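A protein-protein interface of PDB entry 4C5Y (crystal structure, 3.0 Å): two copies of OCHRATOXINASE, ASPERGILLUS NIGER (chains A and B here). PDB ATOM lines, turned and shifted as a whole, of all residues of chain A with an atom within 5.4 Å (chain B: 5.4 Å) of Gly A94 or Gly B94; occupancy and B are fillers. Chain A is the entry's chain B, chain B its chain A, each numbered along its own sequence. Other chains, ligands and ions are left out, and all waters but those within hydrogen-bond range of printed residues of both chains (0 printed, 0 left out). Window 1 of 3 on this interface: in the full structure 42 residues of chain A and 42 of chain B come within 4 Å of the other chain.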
ATOM      1  N   HIS A  89      -9.671 -23.737 -23.832  1.00  0.00           N
ATOM      2  CA  HIS A  89     -10.861 -24.406 -24.287  1.00  0.00           C
ATOM      3  C   HIS A  89     -11.626 -24.898 -23.046  1.00  0.00           C
ATOM      4  O   HIS A  89     -11.021 -25.453 -22.136  1.00  0.00           O
ATOM      5  CB  HIS A  89     -10.487 -25.563 -25.194  1.00  0.00           C
ATOM      6  CG  HIS A  89     -11.654 -26.155 -25.905  1.00  0.00           C
ATOM      7  ND1 HIS A  89     -12.705 -26.740 -25.236  1.00  0.00           N
ATOM      8  CD2 HIS A  89     -11.939 -26.265 -27.221  1.00  0.00           C
ATOM      9  CE1 HIS A  89     -13.590 -27.175 -26.108  1.00  0.00           C
ATOM     10  NE2 HIS A  89     -13.153 -26.894 -27.320  1.00  0.00           N
ATOM     11  N   PRO A  90     -12.958 -24.704 -23.000  1.00  0.00           N
ATOM     12  CA  PRO A  90     -13.675 -24.994 -21.748  1.00  0.00           C
ATOM     13  C   PRO A  90     -13.592 -26.438 -21.311  1.00  0.00           C
ATOM     14  O   PRO A  90     -13.719 -26.712 -20.131  1.00  0.00           O
ATOM     15  CB  PRO A  90     -15.117 -24.625 -22.055  1.00  0.00           C
ATOM     16  CG  PRO A  90     -15.037 -23.719 -23.228  1.00  0.00           C
ATOM     17  CD  PRO A  90     -13.821 -24.080 -24.012  1.00  0.00           C
ATOM     18  N   ALA A  91     -13.404 -27.363 -22.245  1.00  0.00           N
ATOM     19  CA  ALA A  91     -13.098 -28.770 -21.887  1.00  0.00           C
ATOM     20  C   ALA A  91     -11.853 -28.893 -21.015  1.00  0.00           C
ATOM     21  O   ALA A  91     -11.857 -29.590 -20.025  1.00  0.00           O
ATOM     22  CB  ALA A  91     -12.953 -29.645 -23.133  1.00  0.00           C
ATOM     23  N   SER A  92     -10.788 -28.209 -21.380  1.00  0.00           N
ATOM     24  CA  SER A  92      -9.610 -28.261 -20.551  1.00  0.00           C
ATOM     25  C   SER A  92      -9.982 -27.702 -19.197  1.00  0.00           C
ATOM     26  O   SER A  92      -9.688 -28.302 -18.181  1.00  0.00           O
ATOM     27  CB  SER A  92      -8.470 -27.481 -21.172  1.00  0.00           C
ATOM     28  OG  SER A  92      -8.263 -27.912 -22.507  1.00  0.00           O
ATOM     29  N   SER A  93     -10.671 -26.577 -19.179  1.00  0.00           N
ATOM     30  CA  SER A  93     -11.082 -25.965 -17.925  1.00  0.00           C
ATOM     31  C   SER A  93     -11.920 -26.879 -17.088  1.00  0.00           C
ATOM     32  O   SER A  93     -11.733 -26.981 -15.895  1.00  0.00           O
ATOM     33  CB  SER A  93     -11.876 -24.698 -18.196  1.00  0.00           C
ATOM     34  OG  SER A  93     -11.072 -23.778 -18.915  1.00  0.00           O
ATOM     35  N   GLY A  94     -12.876 -27.527 -17.711  1.00  0.00           N
ATOM     36  CA  GLY A  94     -13.788 -28.392 -16.975  1.00  0.00           C
ATOM     37  C   GLY A  94     -13.038 -29.503 -16.273  1.00  0.00           C
ATOM     38  O   GLY A  94     -13.237 -29.733 -15.097  1.00  0.00           O
ATOM     39  N   ALA A  95     -12.172 -30.183 -17.023  1.00  0.00           N
ATOM     40  CA  ALA A  95     -11.370 -31.267 -16.504  1.00  0.00           C
ATOM     41  C   ALA A  95     -10.646 -30.801 -15.267  1.00  0.00           C
ATOM     42  O   ALA A  95     -10.692 -31.444 -14.220  1.00  0.00           O
ATOM     43  CB  ALA A  95     -10.378 -31.727 -17.560  1.00  0.00           C
ATOM     44  N   ARG A  96      -9.963 -29.674 -15.386  1.00  0.00           N
ATOM     45  CA  ARG A  96      -9.209 -29.150 -14.252  1.00  0.00           C
ATOM     46  C   ARG A  96     -10.116 -28.801 -13.088  1.00  0.00           C
ATOM     47  O   ARG A  96      -9.767 -29.031 -11.946  1.00  0.00           O
ATOM     48  CB  ARG A  96      -8.361 -27.927 -14.644  1.00  0.00           C
ATOM     49  CG  ARG A  96      -7.222 -28.245 -15.604  1.00  0.00           C
ATOM     50  CD  ARG A  96      -6.180 -27.136 -15.691  1.00  0.00           C
ATOM     51  NE  ARG A  96      -5.331 -27.352 -16.862  1.00  0.00           N
ATOM     52  CZ  ARG A  96      -5.572 -26.878 -18.086  1.00  0.00           C
ATOM     53  NH1 ARG A  96      -6.647 -26.117 -18.329  1.00  0.00           N
ATOM     54  NH2 ARG A  96      -4.735 -27.167 -19.079  1.00  0.00           N
ATOM     55  N   LEU A  97     -11.282 -28.244 -13.372  1.00  0.00           N
ATOM     56  CA  LEU A  97     -12.161 -27.802 -12.309  1.00  0.00           C
ATOM     57  C   LEU A  97     -12.700 -28.976 -11.504  1.00  0.00           C
ATOM     58  O   LEU A  97     -13.107 -28.820 -10.350  1.00  0.00           O
ATOM     59  CB  LEU A  97     -13.294 -26.966 -12.893  1.00  0.00           C
ATOM     60  CG  LEU A  97     -12.864 -25.549 -13.296  1.00  0.00           C
ATOM     61  CD1 LEU A  97     -13.885 -24.882 -14.196  1.00  0.00           C
ATOM     62  CD2 LEU A  97     -12.655 -24.701 -12.062  1.00  0.00           C
ATOM     63  N   ALA A  98     -12.696 -30.160 -12.111  1.00  0.00           N
ATOM     64  CA  ALA A  98     -13.082 -31.393 -11.413  1.00  0.00           C
ATOM     65  C   ALA A  98     -12.122 -31.658 -10.283  1.00  0.00           C
ATOM     66  O   ALA A  98     -12.543 -31.839  -9.153  1.00  0.00           O
ATOM     67  CB  ALA A  98     -13.082 -32.574 -12.370  1.00  0.00           C
ATOM     68  N   VAL A 122     -20.277 -26.560 -14.695  1.00  0.00           N
ATOM     69  CA  VAL A 122     -19.627 -27.636 -13.968  1.00  0.00           C
ATOM     70  C   VAL A 122     -20.543 -28.172 -12.868  1.00  0.00           C
ATOM     71  O   VAL A 122     -20.512 -29.353 -12.557  1.00  0.00           O
ATOM     72  CB  VAL A 122     -18.305 -27.163 -13.333  1.00  0.00           C
ATOM     73  CG1 VAL A 122     -17.650 -28.284 -12.551  1.00  0.00           C
ATOM     74  CG2 VAL A 122     -17.349 -26.681 -14.405  1.00  0.00           C
ATOM     75  N   HIS B  89     -22.309 -28.017 -22.934  1.00  0.00           N
ATOM     76  CA  HIS B  89     -21.250 -27.055 -22.838  1.00  0.00           C
ATOM     77  C   HIS B  89     -19.970 -27.809 -22.534  1.00  0.00           C
ATOM     78  O   HIS B  89     -19.965 -28.683 -21.675  1.00  0.00           O
ATOM     79  CB  HIS B  89     -21.549 -26.040 -21.740  1.00  0.00           C
ATOM     80  CG  HIS B  89     -20.622 -24.874 -21.746  1.00  0.00           C
ATOM     81  ND1 HIS B  89     -19.271 -25.005 -21.545  1.00  0.00           N
ATOM     82  CD2 HIS B  89     -20.847 -23.556 -21.936  1.00  0.00           C
ATOM     83  CE1 HIS B  89     -18.700 -23.820 -21.593  1.00  0.00           C
ATOM     84  NE2 HIS B  89     -19.636 -22.920 -21.832  1.00  0.00           N
ATOM     85  N   PRO B  90     -18.875 -27.467 -23.219  1.00  0.00           N
ATOM     86  CA  PRO B  90     -17.682 -28.303 -23.085  1.00  0.00           C
ATOM     87  C   PRO B  90     -17.109 -28.354 -21.691  1.00  0.00           C
ATOM     88  O   PRO B  90     -16.439 -29.316 -21.366  1.00  0.00           O
ATOM     89  CB  PRO B  90     -16.677 -27.668 -24.028  1.00  0.00           C
ATOM     90  CG  PRO B  90     -17.493 -26.858 -24.974  1.00  0.00           C
ATOM     91  CD  PRO B  90     -18.727 -26.435 -24.251  1.00  0.00           C
ATOM     92  N   ALA B  91     -17.345 -27.329 -20.883  1.00  0.00           N
ATOM     93  CA  ALA B  91     -17.018 -27.385 -19.453  1.00  0.00           C
ATOM     94  C   ALA B  91     -17.719 -28.545 -18.762  1.00  0.00           C
ATOM     95  O   ALA B  91     -17.110 -29.271 -17.989  1.00  0.00           O
ATOM     96  CB  ALA B  91     -17.350 -26.069 -18.746  1.00  0.00           C
ATOM     97  N   SER B  92     -19.005 -28.718 -19.019  1.00  0.00           N
ATOM     98  CA  SER B  92     -19.701 -29.823 -18.390  1.00  0.00           C
ATOM     99  C   SER B  92     -19.040 -31.102 -18.869  1.00  0.00           C
ATOM    100  O   SER B  92     -18.697 -31.958 -18.074  1.00  0.00           O
ATOM    101  CB  SER B  92     -21.184 -29.804 -18.710  1.00  0.00           C
ATOM    102  OG  SER B  92     -21.735 -28.549 -18.377  1.00  0.00           O
ATOM    103  N   SER B  93     -18.806 -31.197 -20.166  1.00  0.00           N
ATOM    104  CA  SER B  93     -18.138 -32.365 -20.720  1.00  0.00           C
ATOM    105  C   SER B  93     -16.773 -32.611 -20.108  1.00  0.00           C
ATOM    106  O   SER B  93     -16.433 -33.732 -19.768  1.00  0.00           O
ATOM    107  CB  SER B  93     -17.965 -32.211 -22.212  1.00  0.00           C
ATOM    108  OG  SER B  93     -19.222 -32.042 -22.820  1.00  0.00           O
ATOM    109  N   GLY B  94     -15.989 -31.558 -19.970  1.00  0.00           N
ATOM    110  CA  GLY B  94     -14.650 -31.694 -19.428  1.00  0.00           C
ATOM    111  C   GLY B  94     -14.677 -32.259 -18.035  1.00  0.00           C
ATOM    112  O   GLY B  94     -13.975 -33.226 -17.751  1.00  0.00           O
ATOM    113  N   ALA B  95     -15.515 -31.681 -17.176  1.00  0.00           N
ATOM    114  CA  ALA B  95     -15.678 -32.149 -15.803  1.00  0.00           C
ATOM    115  C   ALA B  95     -15.984 -33.640 -15.779  1.00  0.00           C
ATOM    116  O   ALA B  95     -15.322 -34.416 -15.082  1.00  0.00           O
ATOM    117  CB  ALA B  95     -16.792 -31.387 -15.125  1.00  0.00           C
ATOM    118  N   ARG B  96     -16.980 -34.041 -16.561  1.00  0.00           N
ATOM    119  CA  ARG B  96     -17.352 -35.449 -16.608  1.00  0.00           C
ATOM    120  C   ARG B  96     -16.214 -36.321 -17.137  1.00  0.00           C
ATOM    121  O   ARG B  96     -15.982 -37.414 -16.621  1.00  0.00           O
ATOM    122  CB  ARG B  96     -18.606 -35.685 -17.442  1.00  0.00           C
ATOM    123  CG  ARG B  96     -19.861 -35.107 -16.835  1.00  0.00           C
ATOM    124  CD  ARG B  96     -21.146 -35.665 -17.473  1.00  0.00           C
ATOM    125  NE  ARG B  96     -22.300 -34.824 -17.125  1.00  0.00           N
ATOM    126  CZ  ARG B  96     -22.708 -33.760 -17.814  1.00  0.00           C
ATOM    127  NH1 ARG B  96     -22.108 -33.398 -18.949  1.00  0.00           N
ATOM    128  NH2 ARG B  96     -23.736 -33.052 -17.353  1.00  0.00           N
ATOM    129  N   LEU B  97     -15.486 -35.839 -18.142  1.00  0.00           N
ATOM    130  CA  LEU B  97     -14.438 -36.651 -18.754  1.00  0.00           C
ATOM    131  C   LEU B  97     -13.295 -36.914 -17.775  1.00  0.00           C
ATOM    132  O   LEU B  97     -12.539 -37.876 -17.925  1.00  0.00           O
ATOM    133  CB  LEU B  97     -13.928 -35.979 -20.023  1.00  0.00           C
ATOM    134  CG  LEU B  97     -14.893 -36.118 -21.195  1.00  0.00           C
ATOM    135  CD1 LEU B  97     -14.577 -35.145 -22.309  1.00  0.00           C
ATOM    136  CD2 LEU B  97     -14.874 -37.529 -21.736  1.00  0.00           C
ATOM    137  N   ALA B  98     -13.183 -36.054 -16.764  1.00  0.00           N
ATOM    138  CA  ALA B  98     -12.212 -36.249 -15.693  1.00  0.00           C
ATOM    139  C   ALA B  98     -12.517 -37.526 -14.952  1.00  0.00           C
ATOM    140  O   ALA B  98     -11.643 -38.370 -14.812  1.00  0.00           O
ATOM    141  CB  ALA B  98     -12.215 -35.067 -14.720  1.00  0.00           C
ATOM    142  N   VAL B 122      -8.711 -32.272 -23.347  1.00  0.00           N
ATOM    143  CA  VAL B 122      -8.659 -32.850 -22.016  1.00  0.00           C
ATOM    144  C   VAL B 122      -7.284 -33.414 -21.739  1.00  0.00           C
ATOM    145  O   VAL B 122      -6.825 -33.396 -20.599  1.00  0.00           O
ATOM    146  CB  VAL B 122      -9.708 -33.963 -21.849  1.00  0.00           C
ATOM    147  CG1 VAL B 122      -9.620 -34.588 -20.475  1.00  0.00           C
ATOM    148  CG2 VAL B 122     -11.106 -33.406 -22.050  1.00  0.00           C
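His A89 touches Pro B90.
Ala B91 touches Pro A90.
Ala A91 touches Gly B94.
C of Gly A94 touches C of Gly B94, 3.7 Å away.
Ala B95 touches Gly A94.
Ala A95 touches Gly B94.
Ala A95 touches Ala B95 (N to N, 3.7 Å).
Ala B98 touches Ala A95.
Ala B95 touches Ala A98 (O to CB, 3.97 Å).
Ala A98 touches Ala B98.
Printed residues of chain A that touch a printed residue of chain B: His A89, Pro A90, Ala A91, Gly A94, Ala A95 and Ala A98.
Hydrophobic or aromatic side chains of chain A that line the printed part of chain B: His A89, Pro A90, Ala A91, Ala A95 and Ala A98.
Along chain A the printed residues that touch a printed residue of chain B span positions 89 to 98.
His A89 touches Pro B90, and with the chains exchanged Pro A90 touches His B89.
Pro A90 touches Ala B91, and with the chains exchanged Ala A91 touches Pro B90.
Gly B94 touches its own counterpart, Gly A94.
Gly A94 touches Ala B95, and with the chains exchanged Ala A95 touches Gly B94.
Positions printed for both chains: 89, 90, 91, 92, 93, 94, 95, 96, 97, 98 and 122.
Of the 14 pairs that touch across the chains among the printed residues, 14 have their exchanged pair printed and touching as well.
A ring nitrogen (ND1) of His B89 sits at hydrogen-bond distance from the backbone NH (N) of Ala B91, 3.1 Å away.
ND1 of His A89 lies within hydrogen-bond range of N of Ala A91 (3.1 Å).
Of the printed residues of chain B, Pro A90 touches His B89, Pro B90 and Ala B91.
Gly A94 touches three residues of chain B.
Arg A96 touches none of the printed residues of chain B.
Printed residues of chain A within 4 Å of His B89: Pro A90 (3.7 Å).
Of the printed residues of chain A, Ala B95 touches Gly A94 (3.4 Å), Ala A95 (3.7 Å) and Ala A98 (3.97 Å).
Arg B96 touches none of the printed residues of chain A.
The nearest residue of chain A that does not touch Gly B94 is Pro A90 (5.1 Å).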
